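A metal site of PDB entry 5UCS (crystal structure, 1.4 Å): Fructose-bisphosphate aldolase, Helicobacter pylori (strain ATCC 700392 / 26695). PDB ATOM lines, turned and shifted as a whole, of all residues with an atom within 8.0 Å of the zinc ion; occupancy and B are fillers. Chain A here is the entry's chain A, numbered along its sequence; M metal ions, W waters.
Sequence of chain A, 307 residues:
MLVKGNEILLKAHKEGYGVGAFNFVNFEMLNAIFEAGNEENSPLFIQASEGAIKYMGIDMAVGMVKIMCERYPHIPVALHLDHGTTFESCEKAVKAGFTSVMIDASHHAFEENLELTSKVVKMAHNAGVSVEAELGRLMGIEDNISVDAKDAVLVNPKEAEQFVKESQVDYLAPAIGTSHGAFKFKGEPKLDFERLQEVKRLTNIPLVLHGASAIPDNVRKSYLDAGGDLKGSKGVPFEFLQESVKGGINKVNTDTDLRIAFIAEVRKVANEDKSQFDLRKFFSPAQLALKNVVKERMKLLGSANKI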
ATOM      1  N   ASP A  82     -14.070 -19.372  -8.361  1.00  0.00           N
ATOM      2  CA  ASP A  82     -14.908 -19.102  -7.209  1.00  0.00           C
ATOM      3  C   ASP A  82     -15.751 -20.317  -6.881  1.00  0.00           C
ATOM      4  O   ASP A  82     -16.492 -20.803  -7.738  1.00  0.00           O
ATOM      5  CB  ASP A  82     -15.786 -17.904  -7.561  1.00  0.00           C
ATOM      6  CG  ASP A  82     -16.699 -17.472  -6.436  1.00  0.00           C
ATOM      7  OD1 ASP A  82     -16.381 -17.696  -5.241  1.00  0.00           O
ATOM      8  OD2 ASP A  82     -17.761 -16.887  -6.797  1.00  0.00           O
ATOM      9  N   HIS A  83     -15.653 -20.793  -5.647  1.00  0.00           N
ATOM     10  CA  HIS A  83     -16.417 -21.944  -5.181  1.00  0.00           C
ATOM     11  C   HIS A  83     -16.289 -23.141  -6.124  1.00  0.00           C
ATOM     12  O   HIS A  83     -17.278 -23.747  -6.556  1.00  0.00           O
ATOM     13  CB  HIS A  83     -17.872 -21.570  -4.871  1.00  0.00           C
ATOM     14  CG  HIS A  83     -18.011 -20.767  -3.596  1.00  0.00           C
ATOM     15  ND1 HIS A  83     -17.780 -19.411  -3.551  1.00  0.00           N
ATOM     16  CD2 HIS A  83     -18.294 -21.143  -2.327  1.00  0.00           C
ATOM     17  CE1 HIS A  83     -17.929 -18.988  -2.310  1.00  0.00           C
ATOM     18  NE2 HIS A  83     -18.234 -20.007  -1.540  1.00  0.00           N
ATOM     19  N   MET A 102     -10.323 -21.624  -5.749  1.00  0.00           N
ATOM     20  CA  MET A 102     -10.957 -21.916  -4.475  1.00  0.00           C
ATOM     21  C   MET A 102     -11.612 -23.295  -4.499  1.00  0.00           C
ATOM     22  O   MET A 102     -12.413 -23.603  -5.383  1.00  0.00           O
ATOM     23  CB  MET A 102     -11.990 -20.863  -4.111  1.00  0.00           C
ATOM     24  CG  MET A 102     -12.437 -21.005  -2.677  1.00  0.00           C
ATOM     25  SD  MET A 102     -14.198 -21.188  -2.496  1.00  0.00           S
ATOM     26  CE  MET A 102     -14.292 -21.374  -0.709  1.00  0.00           C
ATOM     27  N   ILE A 103     -11.269 -24.127  -3.509  1.00  0.00           N
ATOM     28  CA  ILE A 103     -11.944 -25.387  -3.266  1.00  0.00           C
ATOM     29  C   ILE A 103     -12.846 -25.215  -2.042  1.00  0.00           C
ATOM     30  O   ILE A 103     -12.362 -24.899  -0.939  1.00  0.00           O
ATOM     31  CB  ILE A 103     -10.959 -26.570  -3.140  1.00  0.00           C
ATOM     32  CG1 ILE A 103     -11.705 -27.896  -2.923  1.00  0.00           C
ATOM     33  CG2 ILE A 103      -9.938 -26.325  -2.010  1.00  0.00           C
ATOM     34  CD1 ILE A 103     -12.565 -28.328  -4.121  1.00  0.00           C
ATOM     35  N   ASP A 104     -14.149 -25.374  -2.236  1.00  0.00           N
ATOM     36  CA  ASP A 104     -15.114 -25.284  -1.147  1.00  0.00           C
ATOM     37  C   ASP A 104     -15.537 -26.678  -0.735  1.00  0.00           C
ATOM     38  O   ASP A 104     -16.391 -27.307  -1.367  1.00  0.00           O
ATOM     39  CB  ASP A 104     -16.359 -24.497  -1.537  1.00  0.00           C
ATOM     40  CG  ASP A 104     -17.329 -24.359  -0.403  1.00  0.00           C
ATOM     41  OD1 ASP A 104     -16.932 -24.649   0.759  1.00  0.00           O
ATOM     42  OD2 ASP A 104     -18.490 -23.923  -0.638  1.00  0.00           O
ATOM     43  N   SER A 106     -16.402 -26.897   2.638  1.00  0.00           N
ATOM     44  CA  SER A 106     -16.775 -26.442   3.972  1.00  0.00           C
ATOM     45  C   SER A 106     -18.039 -27.115   4.478  1.00  0.00           C
ATOM     46  O   SER A 106     -18.373 -26.960   5.664  1.00  0.00           O
ATOM     47  CB  SER A 106     -16.925 -24.913   4.008  1.00  0.00           C
ATOM     48  OG  SER A 106     -18.009 -24.494   3.199  1.00  0.00           O
ATOM     49  N   GLU A 132      -7.497 -20.990  -2.276  1.00  0.00           N
ATOM     50  CA  GLU A 132      -8.379 -20.593  -1.197  1.00  0.00           C
ATOM     51  C   GLU A 132      -9.211 -21.801  -0.754  1.00  0.00           C
ATOM     52  O   GLU A 132      -9.623 -22.606  -1.588  1.00  0.00           O
ATOM     53  CB  GLU A 132      -9.333 -19.499  -1.709  1.00  0.00           C
ATOM     54  CG  GLU A 132     -10.321 -18.963  -0.700  1.00  0.00           C
ATOM     55  CD  GLU A 132     -11.289 -17.946  -1.293  1.00  0.00           C
ATOM     56  OE1 GLU A 132     -10.865 -17.104  -2.100  1.00  0.00           O
ATOM     57  OE2 GLU A 132     -12.480 -17.994  -0.922  1.00  0.00           O
ATOM     58  N   ALA A 133      -9.493 -21.892   0.547  1.00  0.00           N
ATOM     59  CA  ALA A 133     -10.449 -22.857   1.087  1.00  0.00           C
ATOM     60  C   ALA A 133     -11.364 -22.139   2.077  1.00  0.00           C
ATOM     61  O   ALA A 133     -11.196 -20.945   2.355  1.00  0.00           O
ATOM     62  CB  ALA A 133      -9.723 -24.030   1.769  1.00  0.00           C
ATOM     63  N   GLU A 134     -12.347 -22.864   2.601  1.00  0.00           N
ATOM     64  CA  GLU A 134     -13.360 -22.294   3.476  1.00  0.00           C
ATOM     65  C   GLU A 134     -13.569 -23.203   4.677  1.00  0.00           C
ATOM     66  O   GLU A 134     -13.503 -24.435   4.545  1.00  0.00           O
ATOM     67  CB  GLU A 134     -14.680 -22.109   2.703  1.00  0.00           C
ATOM     68  CG  GLU A 134     -15.841 -21.478   3.486  1.00  0.00           C
ATOM     69  CD  GLU A 134     -16.882 -20.840   2.578  1.00  0.00           C
ATOM     70  OE1 GLU A 134     -16.786 -20.972   1.328  1.00  0.00           O
ATOM     71  OE2 GLU A 134     -17.814 -20.189   3.102  1.00  0.00           O
ATOM     72  N   LEU A 135     -13.816 -22.609   5.834  1.00  0.00           N
ATOM     73  CA  LEU A 135     -13.932 -23.384   7.062  1.00  0.00           C
ATOM     74  C   LEU A 135     -14.889 -22.711   8.027  1.00  0.00           C
ATOM     75  O   LEU A 135     -14.763 -21.512   8.304  1.00  0.00           O
ATOM     76  CB  LEU A 135     -12.539 -23.507   7.711  1.00  0.00           C
ATOM     77  CG  LEU A 135     -12.457 -24.426   8.917  1.00  0.00           C
ATOM     78  CD1 LEU A 135     -12.689 -25.871   8.492  1.00  0.00           C
ATOM     79  CD2 LEU A 135     -11.115 -24.251   9.633  1.00  0.00           C
ATOM     80  N   ALA A 173     -11.280 -18.591   3.842  1.00  0.00           N
ATOM     81  CA  ALA A 173     -12.551 -17.942   4.115  1.00  0.00           C
ATOM     82  C   ALA A 173     -13.157 -18.527   5.391  1.00  0.00           C
ATOM     83  O   ALA A 173     -13.785 -19.598   5.348  1.00  0.00           O
ATOM     84  CB  ALA A 173     -13.510 -18.158   2.939  1.00  0.00           C
ATOM     85  N   THR A 178     -21.448 -14.111   8.518  1.00  0.00           N
ATOM     86  CA  THR A 178     -22.384 -14.002   7.411  1.00  0.00           C
ATOM     87  C   THR A 178     -23.166 -15.301   7.264  1.00  0.00           C
ATOM     88  O   THR A 178     -22.668 -16.394   7.569  1.00  0.00           O
ATOM     89  CB  THR A 178     -21.676 -13.674   6.091  1.00  0.00           C
ATOM     90  OG1 THR A 178     -20.787 -14.740   5.730  1.00  0.00           O
ATOM     91  CG2 THR A 178     -20.887 -12.376   6.225  1.00  0.00           C
ATOM     92  N   HIS A 180     -24.220 -17.796   4.895  1.00  0.00           N
ATOM     93  CA  HIS A 180     -23.659 -18.118   3.581  1.00  0.00           C
ATOM     94  C   HIS A 180     -23.333 -19.603   3.544  1.00  0.00           C
ATOM     95  O   HIS A 180     -22.884 -20.172   4.540  1.00  0.00           O
ATOM     96  CB  HIS A 180     -22.387 -17.303   3.341  1.00  0.00           C
ATOM     97  CG  HIS A 180     -21.533 -17.836   2.232  1.00  0.00           C
ATOM     98  ND1 HIS A 180     -21.808 -17.602   0.906  1.00  0.00           N
ATOM     99  CD2 HIS A 180     -20.403 -18.597   2.251  1.00  0.00           C
ATOM    100  CE1 HIS A 180     -20.886 -18.184   0.150  1.00  0.00           C
ATOM    101  NE2 HIS A 180     -20.028 -18.800   0.951  1.00  0.00           N
ATOM    102  N   GLY A 181     -23.556 -20.208   2.379  1.00  0.00           N
ATOM    103  CA  GLY A 181     -23.111 -21.562   2.111  1.00  0.00           C
ATOM    104  C   GLY A 181     -23.524 -22.554   3.172  1.00  0.00           C
ATOM    105  O   GLY A 181     -24.712 -22.696   3.465  1.00  0.00           O
ATOM    106  N   ALA A 182     -22.549 -23.239   3.765  1.00  0.00           N
ATOM    107  CA  ALA A 182     -22.801 -24.240   4.793  1.00  0.00           C
ATOM    108  C   ALA A 182     -23.087 -23.639   6.158  1.00  0.00           C
ATOM    109  O   ALA A 182     -23.241 -24.383   7.129  1.00  0.00           O
ATOM    110  CB  ALA A 182     -21.616 -25.196   4.877  1.00  0.00           C
ATOM    111  N   PHE A 183     -23.165 -22.310   6.255  1.00  0.00           N
ATOM    112  CA  PHE A 183     -23.281 -21.600   7.522  1.00  0.00           C
ATOM    113  C   PHE A 183     -24.450 -20.638   7.489  1.00  0.00           C
ATOM    114  O   PHE A 183     -24.398 -19.543   8.057  1.00  0.00           O
ATOM    115  CB  PHE A 183     -21.987 -20.872   7.864  1.00  0.00           C
ATOM    116  CG  PHE A 183     -20.749 -21.599   7.441  1.00  0.00           C
ATOM    117  CD1 PHE A 183     -19.869 -21.026   6.551  1.00  0.00           C
ATOM    118  CD2 PHE A 183     -20.469 -22.867   7.942  1.00  0.00           C
ATOM    119  CE1 PHE A 183     -18.723 -21.694   6.161  1.00  0.00           C
ATOM    120  CE2 PHE A 183     -19.326 -23.544   7.549  1.00  0.00           C
ATOM    121  CZ  PHE A 183     -18.454 -22.956   6.654  1.00  0.00           C
ATOM    122  N   VAL A 208     -10.512 -14.263   3.717  1.00  0.00           N
ATOM    123  CA  VAL A 208     -11.524 -13.994   2.707  1.00  0.00           C
ATOM    124  C   VAL A 208     -12.900 -13.927   3.342  1.00  0.00           C
ATOM    125  O   VAL A 208     -13.227 -14.733   4.225  1.00  0.00           O
ATOM    126  CB  VAL A 208     -11.499 -15.109   1.647  1.00  0.00           C
ATOM    127  CG1 VAL A 208     -12.387 -14.777   0.462  1.00  0.00           C
ATOM    128  CG2 VAL A 208     -10.057 -15.398   1.193  1.00  0.00           C
ATOM    129  N   LEU A 209     -13.708 -12.974   2.892  1.00  0.00           N
ATOM    130  CA  LEU A 209     -15.077 -12.801   3.354  1.00  0.00           C
ATOM    131  C   LEU A 209     -16.040 -13.144   2.229  1.00  0.00           C
ATOM    132  O   LEU A 209     -16.002 -12.511   1.157  1.00  0.00           O
ATOM    133  CB  LEU A 209     -15.312 -11.366   3.823  1.00  0.00           C
ATOM    134  CG  LEU A 209     -16.699 -11.039   4.360  1.00  0.00           C
ATOM    135  CD1 LEU A 209     -16.908 -11.790   5.696  1.00  0.00           C
ATOM    136  CD2 LEU A 209     -16.818  -9.552   4.558  1.00  0.00           C
ATOM    137  N   HIS A 210     -16.898 -14.134   2.482  1.00  0.00           N
ATOM    138  CA  HIS A 210     -17.992 -14.566   1.621  1.00  0.00           C
ATOM    139  C   HIS A 210     -19.324 -14.119   2.221  1.00  0.00           C
ATOM    140  O   HIS A 210     -19.468 -13.974   3.441  1.00  0.00           O
ATOM    141  CB  HIS A 210     -18.078 -16.105   1.522  1.00  0.00           C
ATOM    142  CG  HIS A 210     -16.904 -16.751   0.848  1.00  0.00           C
ATOM    143  ND1 HIS A 210     -16.897 -18.094   0.509  1.00  0.00           N
ATOM    144  CD2 HIS A 210     -15.713 -16.252   0.437  1.00  0.00           C
ATOM    145  CE1 HIS A 210     -15.739 -18.383  -0.079  1.00  0.00           C
ATOM    146  NE2 HIS A 210     -15.023 -17.279  -0.149  1.00  0.00           N
ATOM    147  N   GLY A 211     -20.317 -13.981   1.352  1.00  0.00           N
ATOM    148  CA  GLY A 211     -21.679 -13.747   1.766  1.00  0.00           C
ATOM    149  C   GLY A 211     -21.969 -12.371   2.304  1.00  0.00           C
ATOM    150  O   GLY A 211     -22.967 -12.196   3.011  1.00  0.00           O
ATOM    151  N   ASN A 253     -15.503 -11.096  -1.553  1.00  0.00           N
ATOM    152  CA  ASN A 253     -16.231 -11.582  -2.718  1.00  0.00           C
ATOM    153  C   ASN A 253     -17.432 -10.694  -2.984  1.00  0.00           C
ATOM    154  O   ASN A 253     -18.217 -10.415  -2.091  1.00  0.00           O
ATOM    155  CB  ASN A 253     -16.712 -13.021  -2.474  1.00  0.00           C
ATOM    156  CG  ASN A 253     -15.557 -14.005  -2.466  1.00  0.00           C
ATOM    157  OD1 ASN A 253     -14.408 -13.656  -2.183  1.00  0.00           O
ATOM    158  ND2 ASN A 253     -15.854 -15.249  -2.805  1.00  0.00           N
HETATM  159 ZN    ZN M   1     -18.268 -19.789   0.561  1.00  0.00          ZN
HETATM  160  O   HOH W   1     -19.599 -21.721   0.595  1.00  0.00           O
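The backbone NH of His 83 sits at hydrogen-bond distance from the side-chain sulfur of Met 102.
A ring nitrogen (ND1) of His 83 lies within hydrogen-bond range of the side-chain carboxylate of Asp 82.
A ring nitrogen (NE2) of His 210 sits close to the side-chain amide nitrogen of Asn 253 (3.4 Å).
NE2 of His 210 lies within hydrogen-bond range of OE2 of Glu 132 (2.8 Å).
The backbone carbonyl oxygen (O) of His 210 lies within hydrogen-bond range of the side-chain hydroxyl (OG1) of Thr 178.
Four residues have an atom within 4 Å of the zinc ion: His 83, Glu 134, His 180 and His 210.
The zinc ion is bound by the side-chain carboxylate (OE1) of Glu 134 (2.0 Å), a ring nitrogen (NE2) of His 180 (2.1 Å), a ring nitrogen (NE2) of His 83 (2.1 Å), a ring nitrogen (ND1) of His 210 (2.2 Å) and water W1 (2.3 Å).
The zinc ion has five donor atoms within binding distance.
Slightly farther from the zinc ion lies the side-chain carboxylate (OE2) of Glu 134 (2.6 Å).
Water W1 lies within hydrogen-bond range of the side-chain carboxylate (OD2) of Asp 104 (2.8 Å) and the side-chain carboxylate (OE2) of Glu 134 (3.4 Å).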
